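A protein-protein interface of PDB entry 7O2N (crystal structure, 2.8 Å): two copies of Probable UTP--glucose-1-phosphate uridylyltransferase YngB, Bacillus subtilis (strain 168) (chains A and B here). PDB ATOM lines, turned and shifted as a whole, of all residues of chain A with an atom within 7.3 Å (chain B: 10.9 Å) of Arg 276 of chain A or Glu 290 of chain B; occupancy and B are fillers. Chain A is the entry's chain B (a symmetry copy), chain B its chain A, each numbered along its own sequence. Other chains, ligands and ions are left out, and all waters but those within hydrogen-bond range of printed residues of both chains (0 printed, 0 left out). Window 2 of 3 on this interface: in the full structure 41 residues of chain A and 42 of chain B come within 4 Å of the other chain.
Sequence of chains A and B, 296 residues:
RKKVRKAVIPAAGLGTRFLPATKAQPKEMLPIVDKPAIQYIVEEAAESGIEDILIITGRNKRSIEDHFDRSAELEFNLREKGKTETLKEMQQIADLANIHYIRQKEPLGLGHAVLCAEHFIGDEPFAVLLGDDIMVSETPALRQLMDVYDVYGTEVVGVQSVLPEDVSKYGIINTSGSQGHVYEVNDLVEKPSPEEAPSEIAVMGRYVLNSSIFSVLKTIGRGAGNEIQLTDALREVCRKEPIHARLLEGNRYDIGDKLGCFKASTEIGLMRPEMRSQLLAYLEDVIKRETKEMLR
O of Lys 263 of chain B lies within hydrogen-bond range of OH of Tyr 282 of chain A (3.4 Å).
OH of Tyr 282 of chain B is in hydrogen-bond range of OE2 of Glu 267 of chain A (2.5 Å).
The guanidinium group (NH2) of Arg 289 of chain B lies within salt-bridge range of the side-chain carboxylate (OE2) of Glu 267 of chain A (2.8 Å).
The guanidinium group (NH2) of Arg 276 of chain A lies within salt-bridge range of the side-chain carboxylate (OE1) of Glu 290 of chain B, at 2.7 Å.
Among the printed residues, merely in contact across the chains: Thr 266 of chain A with Phe 262 of chain B, Thr 266 of chain A with Tyr 282 of chain B, Glu 284 of chain A with Ile 287 of chain B, Glu 267 of chain A with Val 286 of chain B, Leu 279 of chain A with Leu 259 of chain B, Gln 278 of chain A with Leu 259 of chain B and Leu 279 of chain A with Phe 262 of chain B.
3 positions are printed for both chains.
Of the 11 pairs that touch across the chains among the printed residues, none has its exchanged pair printed and touching as well.
The backbone carbonyl oxygen (O) of Ile 287 of chain B lies within hydrogen-bond range of the side-chain hydroxyl (OG1) of Thr 291 of chain B (2.8 Å).
NH1 of Arg 289 of chain B is in salt-bridge range of OE2 of Glu 290 of chain B, at 3.4 Å.
The backbone carbonyl oxygen of Leu 270 of chain A lies close to the guanidinium group of Arg 276 of chain A (3.4 Å).
Arg 276 of chain A touches just one residue of chain B: Glu 290 (2.7 Å).
Glu 290 of chain B touches just one residue of chain A: Arg 276 (2.7 Å).
No residue of chain B comes within 4 Å of Pro 273 of chain A.
No residue of chain B comes within 4 Å of Met 275 of chain A.
Ser 277 of chain A touches none of the printed residues of chain B.
Leu 280 of chain A touches none of the printed residues of chain B.
Printed residues of chain A within 4 Å of Ile 287 of chain B: Glu 284.
Printed residues of chain A within 4 Å of Leu 259 of chain B: Gln 278 (3.8 Å) and Leu 279 (3.8 Å).
Printed residues of chain B within 4 Å of Gln 278 of chain A: Leu 259.
Of the printed residues of chain A, Val 286 of chain B touches Glu 267.
The nearest residue of chain A that does not touch Glu 290 of chain B is Leu 280 of chain A (4.4 Å).
Of the 17 printed residues of chain A, 7 touch a printed residue of chain B.
Hydrophobic or aromatic side chains of chain A within 4 Å of the printed part of chain B: Leu 279 and Tyr 282.
Among the printed residues, Asp or Glu carboxylates within 4 Å of a Lys or Arg side-chain nitrogen of the other chain: Glu 267 of chain A with Arg 289 of chain B (2.8 Å) and Arg 276 of chain A with Glu 290 of chain B (2.7 Å).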
ATOM      1  N   THR A 266      -0.533  -8.169 -16.317  1.00  0.00           N
ATOM      2  CA  THR A 266      -1.262  -8.519 -17.525  1.00  0.00           C
ATOM      3  C   THR A 266      -2.113  -9.770 -17.309  1.00  0.00           C
ATOM      4  O   THR A 266      -3.311  -9.763 -17.611  1.00  0.00           O
ATOM      5  CB  THR A 266      -0.289  -8.709 -18.690  1.00  0.00           C
ATOM      6  OG1 THR A 266       0.315  -7.431 -18.866  1.00  0.00           O
ATOM      7  CG2 THR A 266      -0.975  -9.134 -19.968  1.00  0.00           C
ATOM      8  N   GLU A 267      -1.491 -10.836 -16.793  1.00  0.00           N
ATOM      9  CA  GLU A 267      -2.182 -12.105 -16.657  1.00  0.00           C
ATOM     10  C   GLU A 267      -3.316 -12.001 -15.638  1.00  0.00           C
ATOM     11  O   GLU A 267      -4.405 -12.532 -15.860  1.00  0.00           O
ATOM     12  CB  GLU A 267      -1.217 -13.224 -16.286  1.00  0.00           C
ATOM     13  CG  GLU A 267      -0.006 -13.315 -17.193  1.00  0.00           C
ATOM     14  CD  GLU A 267      -0.259 -13.871 -18.577  1.00  0.00           C
ATOM     15  OE1 GLU A 267      -1.375 -14.346 -18.815  1.00  0.00           O
ATOM     16  OE2 GLU A 267       0.653 -13.791 -19.412  1.00  0.00           O
ATOM     17  N   GLY A 269      -4.743  -9.304 -14.768  1.00  0.00           N
ATOM     18  CA  GLY A 269      -5.644  -8.330 -15.358  1.00  0.00           C
ATOM     19  C   GLY A 269      -6.673  -9.054 -16.208  1.00  0.00           C
ATOM     20  O   GLY A 269      -7.878  -8.795 -16.110  1.00  0.00           O
ATOM     21  N   LEU A 270      -6.154 -10.015 -16.983  1.00  0.00           N
ATOM     22  CA  LEU A 270      -6.955 -10.822 -17.894  1.00  0.00           C
ATOM     23  C   LEU A 270      -7.951 -11.684 -17.133  1.00  0.00           C
ATOM     24  O   LEU A 270      -8.848 -12.237 -17.743  1.00  0.00           O
ATOM     25  CB  LEU A 270      -6.049 -11.661 -18.794  1.00  0.00           C
ATOM     26  CG  LEU A 270      -5.371 -10.860 -19.898  1.00  0.00           C
ATOM     27  CD1 LEU A 270      -4.186 -11.598 -20.508  1.00  0.00           C
ATOM     28  CD2 LEU A 270      -6.387 -10.401 -20.939  1.00  0.00           C
ATOM     29  N   MET A 271      -7.825 -11.757 -15.810  1.00  0.00           N
ATOM     30  CA  MET A 271      -8.767 -12.553 -15.043  1.00  0.00           C
ATOM     31  C   MET A 271      -9.942 -11.689 -14.588  1.00  0.00           C
ATOM     32  O   MET A 271     -10.970 -12.197 -14.140  1.00  0.00           O
ATOM     33  CB  MET A 271      -8.108 -13.227 -13.840  1.00  0.00           C
ATOM     34  CG  MET A 271      -6.874 -14.051 -14.179  1.00  0.00           C
ATOM     35  SD  MET A 271      -6.367 -15.012 -12.731  1.00  0.00           S
ATOM     36  CE  MET A 271      -7.417 -16.448 -12.972  1.00  0.00           C
ATOM     37  N   ARG A 272      -9.817 -10.376 -14.773  1.00  0.00           N
ATOM     38  CA  ARG A 272     -10.915  -9.517 -14.365  1.00  0.00           C
ATOM     39  C   ARG A 272     -11.800  -9.200 -15.565  1.00  0.00           C
ATOM     40  O   ARG A 272     -11.348  -8.605 -16.541  1.00  0.00           O
ATOM     41  CB  ARG A 272     -10.413  -8.332 -13.534  1.00  0.00           C
ATOM     42  CG  ARG A 272     -10.393  -8.652 -12.047  1.00  0.00           C
ATOM     43  CD  ARG A 272      -9.106  -8.243 -11.380  1.00  0.00           C
ATOM     44  NE  ARG A 272      -9.183  -6.848 -10.991  1.00  0.00           N
ATOM     45  CZ  ARG A 272      -8.337  -6.320 -10.131  1.00  0.00           C
ATOM     46  NH1 ARG A 272      -7.375  -7.066  -9.609  1.00  0.00           N
ATOM     47  NH2 ARG A 272      -8.458  -5.051  -9.796  1.00  0.00           N
ATOM     48  N   PRO A 273     -13.080  -9.630 -15.530  1.00  0.00           N
ATOM     49  CA  PRO A 273     -14.002  -9.456 -16.654  1.00  0.00           C
ATOM     50  C   PRO A 273     -14.041  -8.027 -17.198  1.00  0.00           C
ATOM     51  O   PRO A 273     -14.123  -7.817 -18.410  1.00  0.00           O
ATOM     52  CB  PRO A 273     -15.375  -9.883 -16.098  1.00  0.00           C
ATOM     53  CG  PRO A 273     -15.173  -9.958 -14.598  1.00  0.00           C
ATOM     54  CD  PRO A 273     -13.710 -10.303 -14.392  1.00  0.00           C
ATOM     55  N   GLU A 274     -13.957  -7.054 -16.291  1.00  0.00           N
ATOM     56  CA  GLU A 274     -14.021  -5.651 -16.669  1.00  0.00           C
ATOM     57  C   GLU A 274     -12.804  -5.264 -17.519  1.00  0.00           C
ATOM     58  O   GLU A 274     -12.938  -4.467 -18.441  1.00  0.00           O
ATOM     59  CB  GLU A 274     -14.320  -4.738 -15.472  1.00  0.00           C
ATOM     60  CG  GLU A 274     -13.325  -4.842 -14.319  1.00  0.00           C
ATOM     61  CD  GLU A 274     -13.375  -6.067 -13.406  1.00  0.00           C
ATOM     62  OE1 GLU A 274     -13.985  -7.087 -13.806  1.00  0.00           O
ATOM     63  OE2 GLU A 274     -12.776  -6.018 -12.286  1.00  0.00           O
ATOM     64  N   MET A 275     -11.630  -5.854 -17.253  1.00  0.00           N
ATOM     65  CA  MET A 275     -10.450  -5.484 -18.022  1.00  0.00           C
ATOM     66  C   MET A 275     -10.064  -6.517 -19.079  1.00  0.00           C
ATOM     67  O   MET A 275      -9.285  -6.204 -19.970  1.00  0.00           O
ATOM     68  CB  MET A 275      -9.213  -5.092 -17.199  1.00  0.00           C
ATOM     69  CG  MET A 275      -9.243  -5.442 -15.732  1.00  0.00           C
ATOM     70  SD  MET A 275      -8.085  -4.472 -14.717  1.00  0.00           S
ATOM     71  CE  MET A 275      -7.964  -2.939 -15.656  1.00  0.00           C
ATOM     72  N   ARG A 276     -10.622  -7.728 -19.022  1.00  0.00           N
ATOM     73  CA  ARG A 276     -10.123  -8.788 -19.889  1.00  0.00           C
ATOM     74  C   ARG A 276     -10.202  -8.384 -21.369  1.00  0.00           C
ATOM     75  O   ARG A 276      -9.235  -8.464 -22.138  1.00  0.00           O
ATOM     76  CB  ARG A 276     -10.866 -10.099 -19.640  1.00  0.00           C
ATOM     77  CG  ARG A 276     -10.409 -11.199 -20.588  1.00  0.00           C
ATOM     78  CD  ARG A 276     -10.839 -12.606 -20.234  1.00  0.00           C
ATOM     79  NE  ARG A 276     -10.464 -13.450 -21.348  1.00  0.00           N
ATOM     80  CZ  ARG A 276      -9.352 -14.183 -21.434  1.00  0.00           C
ATOM     81  NH1 ARG A 276      -8.478 -14.214 -20.441  1.00  0.00           N
ATOM     82  NH2 ARG A 276      -9.113 -14.881 -22.532  1.00  0.00           N
ATOM     83  N   SER A 277     -11.392  -7.954 -21.792  1.00  0.00           N
ATOM     84  CA  SER A 277     -11.588  -7.684 -23.205  1.00  0.00           C
ATOM     85  C   SER A 277     -10.883  -6.385 -23.600  1.00  0.00           C
ATOM     86  O   SER A 277     -10.284  -6.317 -24.668  1.00  0.00           O
ATOM     87  CB  SER A 277     -13.048  -7.693 -23.580  1.00  0.00           C
ATOM     88  OG  SER A 277     -13.683  -8.877 -23.125  1.00  0.00           O
ATOM     89  N   GLN A 278     -10.924  -5.364 -22.734  1.00  0.00           N
ATOM     90  CA  GLN A 278     -10.278  -4.099 -23.040  1.00  0.00           C
ATOM     91  C   GLN A 278      -8.788  -4.335 -23.270  1.00  0.00           C
ATOM     92  O   GLN A 278      -8.185  -3.730 -24.147  1.00  0.00           O
ATOM     93  CB  GLN A 278     -10.479  -3.116 -21.895  1.00  0.00           C
ATOM     94  CG  GLN A 278     -11.932  -2.844 -21.573  1.00  0.00           C
ATOM     95  CD  GLN A 278     -12.506  -2.185 -22.791  1.00  0.00           C
ATOM     96  OE1 GLN A 278     -13.710  -2.264 -23.031  1.00  0.00           O
ATOM     97  NE2 GLN A 278     -11.627  -1.566 -23.576  1.00  0.00           N
ATOM     98  N   LEU A 279      -8.226  -5.258 -22.492  1.00  0.00           N
ATOM     99  CA  LEU A 279      -6.797  -5.524 -22.456  1.00  0.00           C
ATOM    100  C   LEU A 279      -6.406  -6.178 -23.770  1.00  0.00           C
ATOM    101  O   LEU A 279      -5.574  -5.647 -24.501  1.00  0.00           O
ATOM    102  CB  LEU A 279      -6.501  -6.455 -21.268  1.00  0.00           C
ATOM    103  CG  LEU A 279      -5.495  -5.982 -20.209  1.00  0.00           C
ATOM    104  CD1 LEU A 279      -5.448  -4.470 -20.072  1.00  0.00           C
ATOM    105  CD2 LEU A 279      -5.761  -6.620 -18.852  1.00  0.00           C
ATOM    106  N   LEU A 280      -7.030  -7.330 -24.044  1.00  0.00           N
ATOM    107  CA  LEU A 280      -6.777  -8.145 -25.220  1.00  0.00           C
ATOM    108  C   LEU A 280      -6.935  -7.301 -26.488  1.00  0.00           C
ATOM    109  O   LEU A 280      -6.044  -7.270 -27.335  1.00  0.00           O
ATOM    110  CB  LEU A 280      -7.762  -9.315 -25.163  1.00  0.00           C
ATOM    111  CG  LEU A 280      -7.185 -10.677 -24.789  1.00  0.00           C
ATOM    112  CD1 LEU A 280      -5.778 -10.565 -24.240  1.00  0.00           C
ATOM    113  CD2 LEU A 280      -8.068 -11.416 -23.808  1.00  0.00           C
ATOM    114  N   ALA A 281      -8.052  -6.573 -26.593  1.00  0.00           N
ATOM    115  CA  ALA A 281      -8.263  -5.660 -27.711  1.00  0.00           C
ATOM    116  C   ALA A 281      -7.047  -4.760 -27.865  1.00  0.00           C
ATOM    117  O   ALA A 281      -6.519  -4.658 -28.957  1.00  0.00           O
ATOM    118  CB  ALA A 281      -9.494  -4.818 -27.506  1.00  0.00           C
ATOM    119  N   TYR A 282      -6.623  -4.129 -26.758  1.00  0.00           N
ATOM    120  CA  TYR A 282      -5.500  -3.209 -26.770  1.00  0.00           C
ATOM    121  C   TYR A 282      -4.222  -3.904 -27.237  1.00  0.00           C
ATOM    122  O   TYR A 282      -3.420  -3.286 -27.947  1.00  0.00           O
ATOM    123  CB  TYR A 282      -5.221  -2.602 -25.397  1.00  0.00           C
ATOM    124  CG  TYR A 282      -3.953  -1.791 -25.384  1.00  0.00           C
ATOM    125  CD1 TYR A 282      -3.838  -0.631 -26.142  1.00  0.00           C
ATOM    126  CD2 TYR A 282      -2.856  -2.207 -24.645  1.00  0.00           C
ATOM    127  CE1 TYR A 282      -2.673   0.113 -26.145  1.00  0.00           C
ATOM    128  CE2 TYR A 282      -1.680  -1.470 -24.631  1.00  0.00           C
ATOM    129  CZ  TYR A 282      -1.595  -0.310 -25.383  1.00  0.00           C
ATOM    130  OH  TYR A 282      -0.427   0.389 -25.401  1.00  0.00           O
ATOM    131  N   GLU A 284      -4.006  -6.679 -29.195  1.00  0.00           N
ATOM    132  CA  GLU A 284      -4.147  -6.861 -30.633  1.00  0.00           C
ATOM    133  C   GLU A 284      -3.739  -5.560 -31.351  1.00  0.00           C
ATOM    134  O   GLU A 284      -2.869  -5.579 -32.230  1.00  0.00           O
ATOM    135  CB  GLU A 284      -5.524  -7.420 -31.006  1.00  0.00           C
ATOM    136  CG  GLU A 284      -5.814  -8.804 -30.462  1.00  0.00           C
ATOM    137  CD  GLU A 284      -7.283  -9.239 -30.387  1.00  0.00           C
ATOM    138  OE1 GLU A 284      -8.203  -8.437 -30.721  1.00  0.00           O
ATOM    139  OE2 GLU A 284      -7.527 -10.400 -29.976  1.00  0.00           O
ATOM    140  N   LEU B 259      -6.710   1.557 -16.671  1.00  0.00           N
ATOM    141  CA  LEU B 259      -6.401   1.138 -18.026  1.00  0.00           C
ATOM    142  C   LEU B 259      -5.443   2.124 -18.685  1.00  0.00           C
ATOM    143  O   LEU B 259      -4.408   1.729 -19.223  1.00  0.00           O
ATOM    144  CB  LEU B 259      -7.704   1.089 -18.805  1.00  0.00           C
ATOM    145  CG  LEU B 259      -7.720   0.146 -19.998  1.00  0.00           C
ATOM    146  CD1 LEU B 259      -7.355  -1.265 -19.545  1.00  0.00           C
ATOM    147  CD2 LEU B 259      -9.113   0.164 -20.629  1.00  0.00           C
ATOM    148  N   PHE B 262      -1.934   1.352 -17.763  1.00  0.00           N
ATOM    149  CA  PHE B 262      -1.425   0.156 -18.391  1.00  0.00           C
ATOM    150  C   PHE B 262      -0.988   0.493 -19.813  1.00  0.00           C
ATOM    151  O   PHE B 262       0.121   0.151 -20.217  1.00  0.00           O
ATOM    152  CB  PHE B 262      -2.479  -0.946 -18.376  1.00  0.00           C
ATOM    153  CG  PHE B 262      -1.974  -2.235 -18.961  1.00  0.00           C
ATOM    154  CD1 PHE B 262      -1.297  -3.146 -18.171  1.00  0.00           C
ATOM    155  CD2 PHE B 262      -2.127  -2.507 -20.318  1.00  0.00           C
ATOM    156  CE1 PHE B 262      -0.764  -4.295 -18.740  1.00  0.00           C
ATOM    157  CE2 PHE B 262      -1.627  -3.672 -20.872  1.00  0.00           C
ATOM    158  CZ  PHE B 262      -0.945  -4.563 -20.079  1.00  0.00           C
ATOM    159  N   LYS B 263      -1.851   1.183 -20.563  1.00  0.00           N
ATOM    160  CA  LYS B 263      -1.510   1.571 -21.918  1.00  0.00           C
ATOM    161  C   LYS B 263      -0.248   2.427 -21.908  1.00  0.00           C
ATOM    162  O   LYS B 263       0.657   2.208 -22.704  1.00  0.00           O
ATOM    163  CB  LYS B 263      -2.677   2.290 -22.595  1.00  0.00           C
ATOM    164  CG  LYS B 263      -3.863   1.398 -22.963  1.00  0.00           C
ATOM    165  CD  LYS B 263      -4.982   2.209 -23.551  1.00  0.00           C
ATOM    166  CE  LYS B 263      -6.089   1.384 -24.156  1.00  0.00           C
ATOM    167  NZ  LYS B 263      -7.237   1.330 -23.234  1.00  0.00           N
ATOM    168  N   ALA B 281       7.762  -9.316 -27.718  1.00  0.00           N
ATOM    169  CA  ALA B 281       7.711 -10.765 -27.771  1.00  0.00           C
ATOM    170  C   ALA B 281       6.640 -11.266 -26.822  1.00  0.00           C
ATOM    171  O   ALA B 281       5.804 -12.057 -27.239  1.00  0.00           O
ATOM    172  CB  ALA B 281       9.028 -11.372 -27.404  1.00  0.00           C
ATOM    173  N   TYR B 282       6.669 -10.777 -25.571  1.00  0.00           N
ATOM    174  CA  TYR B 282       5.712 -11.193 -24.550  1.00  0.00           C
ATOM    175  C   TYR B 282       4.286 -10.900 -25.001  1.00  0.00           C
ATOM    176  O   TYR B 282       3.393 -11.707 -24.747  1.00  0.00           O
ATOM    177  CB  TYR B 282       5.952 -10.531 -23.186  1.00  0.00           C
ATOM    178  CG  TYR B 282       4.818 -10.771 -22.220  1.00  0.00           C
ATOM    179  CD1 TYR B 282       4.544 -12.043 -21.734  1.00  0.00           C
ATOM    180  CD2 TYR B 282       3.976  -9.735 -21.841  1.00  0.00           C
ATOM    181  CE1 TYR B 282       3.469 -12.275 -20.883  1.00  0.00           C
ATOM    182  CE2 TYR B 282       2.881  -9.949 -21.021  1.00  0.00           C
ATOM    183  CZ  TYR B 282       2.626 -11.226 -20.536  1.00  0.00           C
ATOM    184  OH  TYR B 282       1.546 -11.426 -19.715  1.00  0.00           O
ATOM    185  N   LEU B 283       4.077  -9.746 -25.649  1.00  0.00           N
ATOM    186  CA  LEU B 283       2.725  -9.386 -26.049  1.00  0.00           C
ATOM    187  C   LEU B 283       2.244 -10.290 -27.194  1.00  0.00           C
ATOM    188  O   LEU B 283       1.119 -10.802 -27.166  1.00  0.00           O
ATOM    189  CB  LEU B 283       2.672  -7.904 -26.426  1.00  0.00           C
ATOM    190  CG  LEU B 283       3.098  -6.926 -25.341  1.00  0.00           C
ATOM    191  CD1 LEU B 283       3.059  -5.506 -25.863  1.00  0.00           C
ATOM    192  CD2 LEU B 283       2.211  -7.057 -24.125  1.00  0.00           C
ATOM    193  N   GLU B 284       3.106 -10.506 -28.198  1.00  0.00           N
ATOM    194  CA  GLU B 284       2.783 -11.466 -29.244  1.00  0.00           C
ATOM    195  C   GLU B 284       2.385 -12.794 -28.593  1.00  0.00           C
ATOM    196  O   GLU B 284       1.323 -13.337 -28.877  1.00  0.00           O
ATOM    197  CB  GLU B 284       3.912 -11.578 -30.272  1.00  0.00           C
ATOM    198  CG  GLU B 284       4.108 -10.317 -31.099  1.00  0.00           C
ATOM    199  CD  GLU B 284       5.367 -10.267 -31.956  1.00  0.00           C
ATOM    200  OE1 GLU B 284       6.331 -11.012 -31.648  1.00  0.00           O
ATOM    201  OE2 GLU B 284       5.390  -9.475 -32.945  1.00  0.00           O
ATOM    202  N   ASP B 285       3.214 -13.278 -27.664  1.00  0.00           N
ATOM    203  CA  ASP B 285       3.041 -14.545 -26.988  1.00  0.00           C
ATOM    204  C   ASP B 285       1.687 -14.626 -26.292  1.00  0.00           C
ATOM    205  O   ASP B 285       1.064 -15.680 -26.309  1.00  0.00           O
ATOM    206  CB  ASP B 285       4.159 -14.750 -25.972  1.00  0.00           C
ATOM    207  CG  ASP B 285       5.114 -15.867 -26.351  1.00  0.00           C
ATOM    208  OD1 ASP B 285       4.757 -17.042 -26.082  1.00  0.00           O
ATOM    209  OD2 ASP B 285       6.198 -15.564 -26.926  1.00  0.00           O
ATOM    210  N   VAL B 286       1.255 -13.542 -25.644  1.00  0.00           N
ATOM    211  CA  VAL B 286      -0.008 -13.580 -24.919  1.00  0.00           C
ATOM    212  C   VAL B 286      -1.151 -13.864 -25.892  1.00  0.00           C
ATOM    213  O   VAL B 286      -1.969 -14.742 -25.629  1.00  0.00           O
ATOM    214  CB  VAL B 286      -0.268 -12.297 -24.099  1.00  0.00           C
ATOM    215  CG1 VAL B 286      -1.749 -12.093 -23.790  1.00  0.00           C
ATOM    216  CG2 VAL B 286       0.512 -12.303 -22.804  1.00  0.00           C
ATOM    217  N   ILE B 287      -1.185 -13.125 -27.012  1.00  0.00           N
ATOM    218  CA  ILE B 287      -2.220 -13.275 -28.024  1.00  0.00           C
ATOM    219  C   ILE B 287      -2.165 -14.661 -28.671  1.00  0.00           C
ATOM    220  O   ILE B 287      -3.203 -15.311 -28.795  1.00  0.00           O
ATOM    221  CB  ILE B 287      -2.165 -12.123 -29.048  1.00  0.00           C
ATOM    222  CG1 ILE B 287      -2.938 -10.910 -28.531  1.00  0.00           C
ATOM    223  CG2 ILE B 287      -2.667 -12.541 -30.429  1.00  0.00           C
ATOM    224  CD1 ILE B 287      -2.075  -9.705 -28.344  1.00  0.00           C
ATOM    225  N   LYS B 288      -0.971 -15.104 -29.099  1.00  0.00           N
ATOM    226  CA  LYS B 288      -0.846 -16.458 -29.616  1.00  0.00           C
ATOM    227  C   LYS B 288      -1.491 -17.448 -28.635  1.00  0.00           C
ATOM    228  O   LYS B 288      -2.352 -18.238 -29.018  1.00  0.00           O
ATOM    229  CB  LYS B 288       0.591 -16.762 -30.051  1.00  0.00           C
ATOM    230  N   ARG B 289      -1.136 -17.362 -27.350  1.00  0.00           N
ATOM    231  CA  ARG B 289      -1.639 -18.308 -26.367  1.00  0.00           C
ATOM    232  C   ARG B 289      -3.157 -18.185 -26.194  1.00  0.00           C
ATOM    233  O   ARG B 289      -3.842 -19.181 -25.936  1.00  0.00           O
ATOM    234  CB  ARG B 289      -0.833 -18.184 -25.074  1.00  0.00           C
ATOM    235  CG  ARG B 289      -1.357 -18.987 -23.888  1.00  0.00           C
ATOM    236  CD  ARG B 289      -0.399 -18.977 -22.698  1.00  0.00           C
ATOM    237  NE  ARG B 289       0.208 -17.682 -22.378  1.00  0.00           N
ATOM    238  CZ  ARG B 289      -0.412 -16.635 -21.823  1.00  0.00           C
ATOM    239  NH1 ARG B 289      -1.704 -16.672 -21.513  1.00  0.00           N
ATOM    240  NH2 ARG B 289       0.281 -15.532 -21.618  1.00  0.00           N
ATOM    241  N   GLU B 290      -3.692 -16.975 -26.371  1.00  0.00           N
ATOM    242  CA  GLU B 290      -5.109 -16.762 -26.116  1.00  0.00           C
ATOM    243  C   GLU B 290      -5.934 -17.232 -27.315  1.00  0.00           C
ATOM    244  O   GLU B 290      -7.092 -17.607 -27.151  1.00  0.00           O
ATOM    245  CB  GLU B 290      -5.390 -15.303 -25.737  1.00  0.00           C
ATOM    246  CG  GLU B 290      -5.040 -14.946 -24.296  1.00  0.00           C
ATOM    247  CD  GLU B 290      -5.486 -15.886 -23.177  1.00  0.00           C
ATOM    248  OE1 GLU B 290      -6.530 -15.610 -22.544  1.00  0.00           O
ATOM    249  OE2 GLU B 290      -4.760 -16.874 -22.900  1.00  0.00           O
ATOM    250  N   THR B 291      -5.336 -17.196 -28.515  1.00  0.00           N
ATOM    251  CA  THR B 291      -5.972 -17.719 -29.711  1.00  0.00           C
ATOM    252  C   THR B 291      -6.087 -19.233 -29.579  1.00  0.00           C
ATOM    253  O   THR B 291      -7.210 -19.744 -29.619  1.00  0.00           O
ATOM    254  CB  THR B 291      -5.191 -17.356 -30.983  1.00  0.00           C
ATOM    255  OG1 THR B 291      -4.848 -15.971 -30.945  1.00  0.00           O
ATOM    256  CG2 THR B 291      -5.940 -17.680 -32.257  1.00  0.00           C
ATOM    257  N   LYS B 292      -4.933 -19.920 -29.409  1.00  0.00           N
ATOM    258  CA  LYS B 292      -4.885 -21.363 -29.217  1.00  0.00           C
ATOM    259  C   LYS B 292      -5.973 -21.793 -28.227  1.00  0.00           C
ATOM    260  O   LYS B 292      -6.847 -22.580 -28.584  1.00  0.00           O
ATOM    261  CB  LYS B 292      -3.483 -21.847 -28.834  1.00  0.00           C
ATOM    262  N   GLU B 293      -5.951 -21.248 -26.998  1.00  0.00           N
ATOM    263  CA  GLU B 293      -6.881 -21.672 -25.956  1.00  0.00           C
ATOM    264  C   GLU B 293      -8.320 -21.485 -26.428  1.00  0.00           C
ATOM    265  O   GLU B 293      -9.209 -22.215 -25.998  1.00  0.00           O
ATOM    266  CB  GLU B 293      -6.624 -20.971 -24.620  1.00  0.00           C
ATOM    267  N   MET B 294      -8.530 -20.529 -27.339  1.00  0.00           N
ATOM    268  CA  MET B 294      -9.863 -20.132 -27.768  1.00  0.00           C
ATOM    269  C   MET B 294     -10.399 -21.093 -28.832  1.00  0.00           C
ATOM    270  O   MET B 294     -11.580 -21.452 -28.801  1.00  0.00           O
ATOM    271  CB  MET B 294      -9.873 -18.692 -28.297  1.00  0.00           C
ATOM    272  CG  MET B 294     -11.178 -17.957 -27.995  1.00  0.00           C
ATOM    273  SD  MET B 294     -11.863 -17.007 -29.378  1.00  0.00           S
ATOM    274  CE  MET B 294     -11.246 -17.970 -30.757  1.00  0.00           C
ATOM    275  N   LEU B 295      -9.526 -21.527 -29.757  1.00  0.00           N
ATOM    276  CA  LEU B 295      -9.936 -22.388 -30.860  1.00  0.00           C
ATOM    277  C   LEU B 295     -10.396 -23.753 -30.325  1.00  0.00           C
ATOM    278  O   LEU B 295     -11.393 -24.298 -30.794  1.00  0.00           O
ATOM    279  CB  LEU B 295      -8.825 -22.480 -31.921  1.00  0.00           C
ATOM    280  CG  LEU B 295      -8.009 -23.783 -31.937  1.00  0.00           C
ATOM    281  CD1 LEU B 295      -8.590 -24.808 -32.908  1.00  0.00           C
ATOM    282  CD2 LEU B 295      -6.532 -23.537 -32.234  1.00  0.00           C
ATOM    283  N   ARG B 296      -9.679 -24.297 -29.328  1.00  0.00           N
ATOM    284  CA  ARG B 296     -10.244 -25.321 -28.464  1.00  0.00           C
ATOM    285  C   ARG B 296     -11.228 -24.617 -27.521  1.00  0.00           C
ATOM    286  O   ARG B 296     -12.231 -25.246 -27.158  1.00  0.00           O
ATOM    287  CB  ARG B 296      -9.150 -26.082 -27.702  1.00  0.00           C
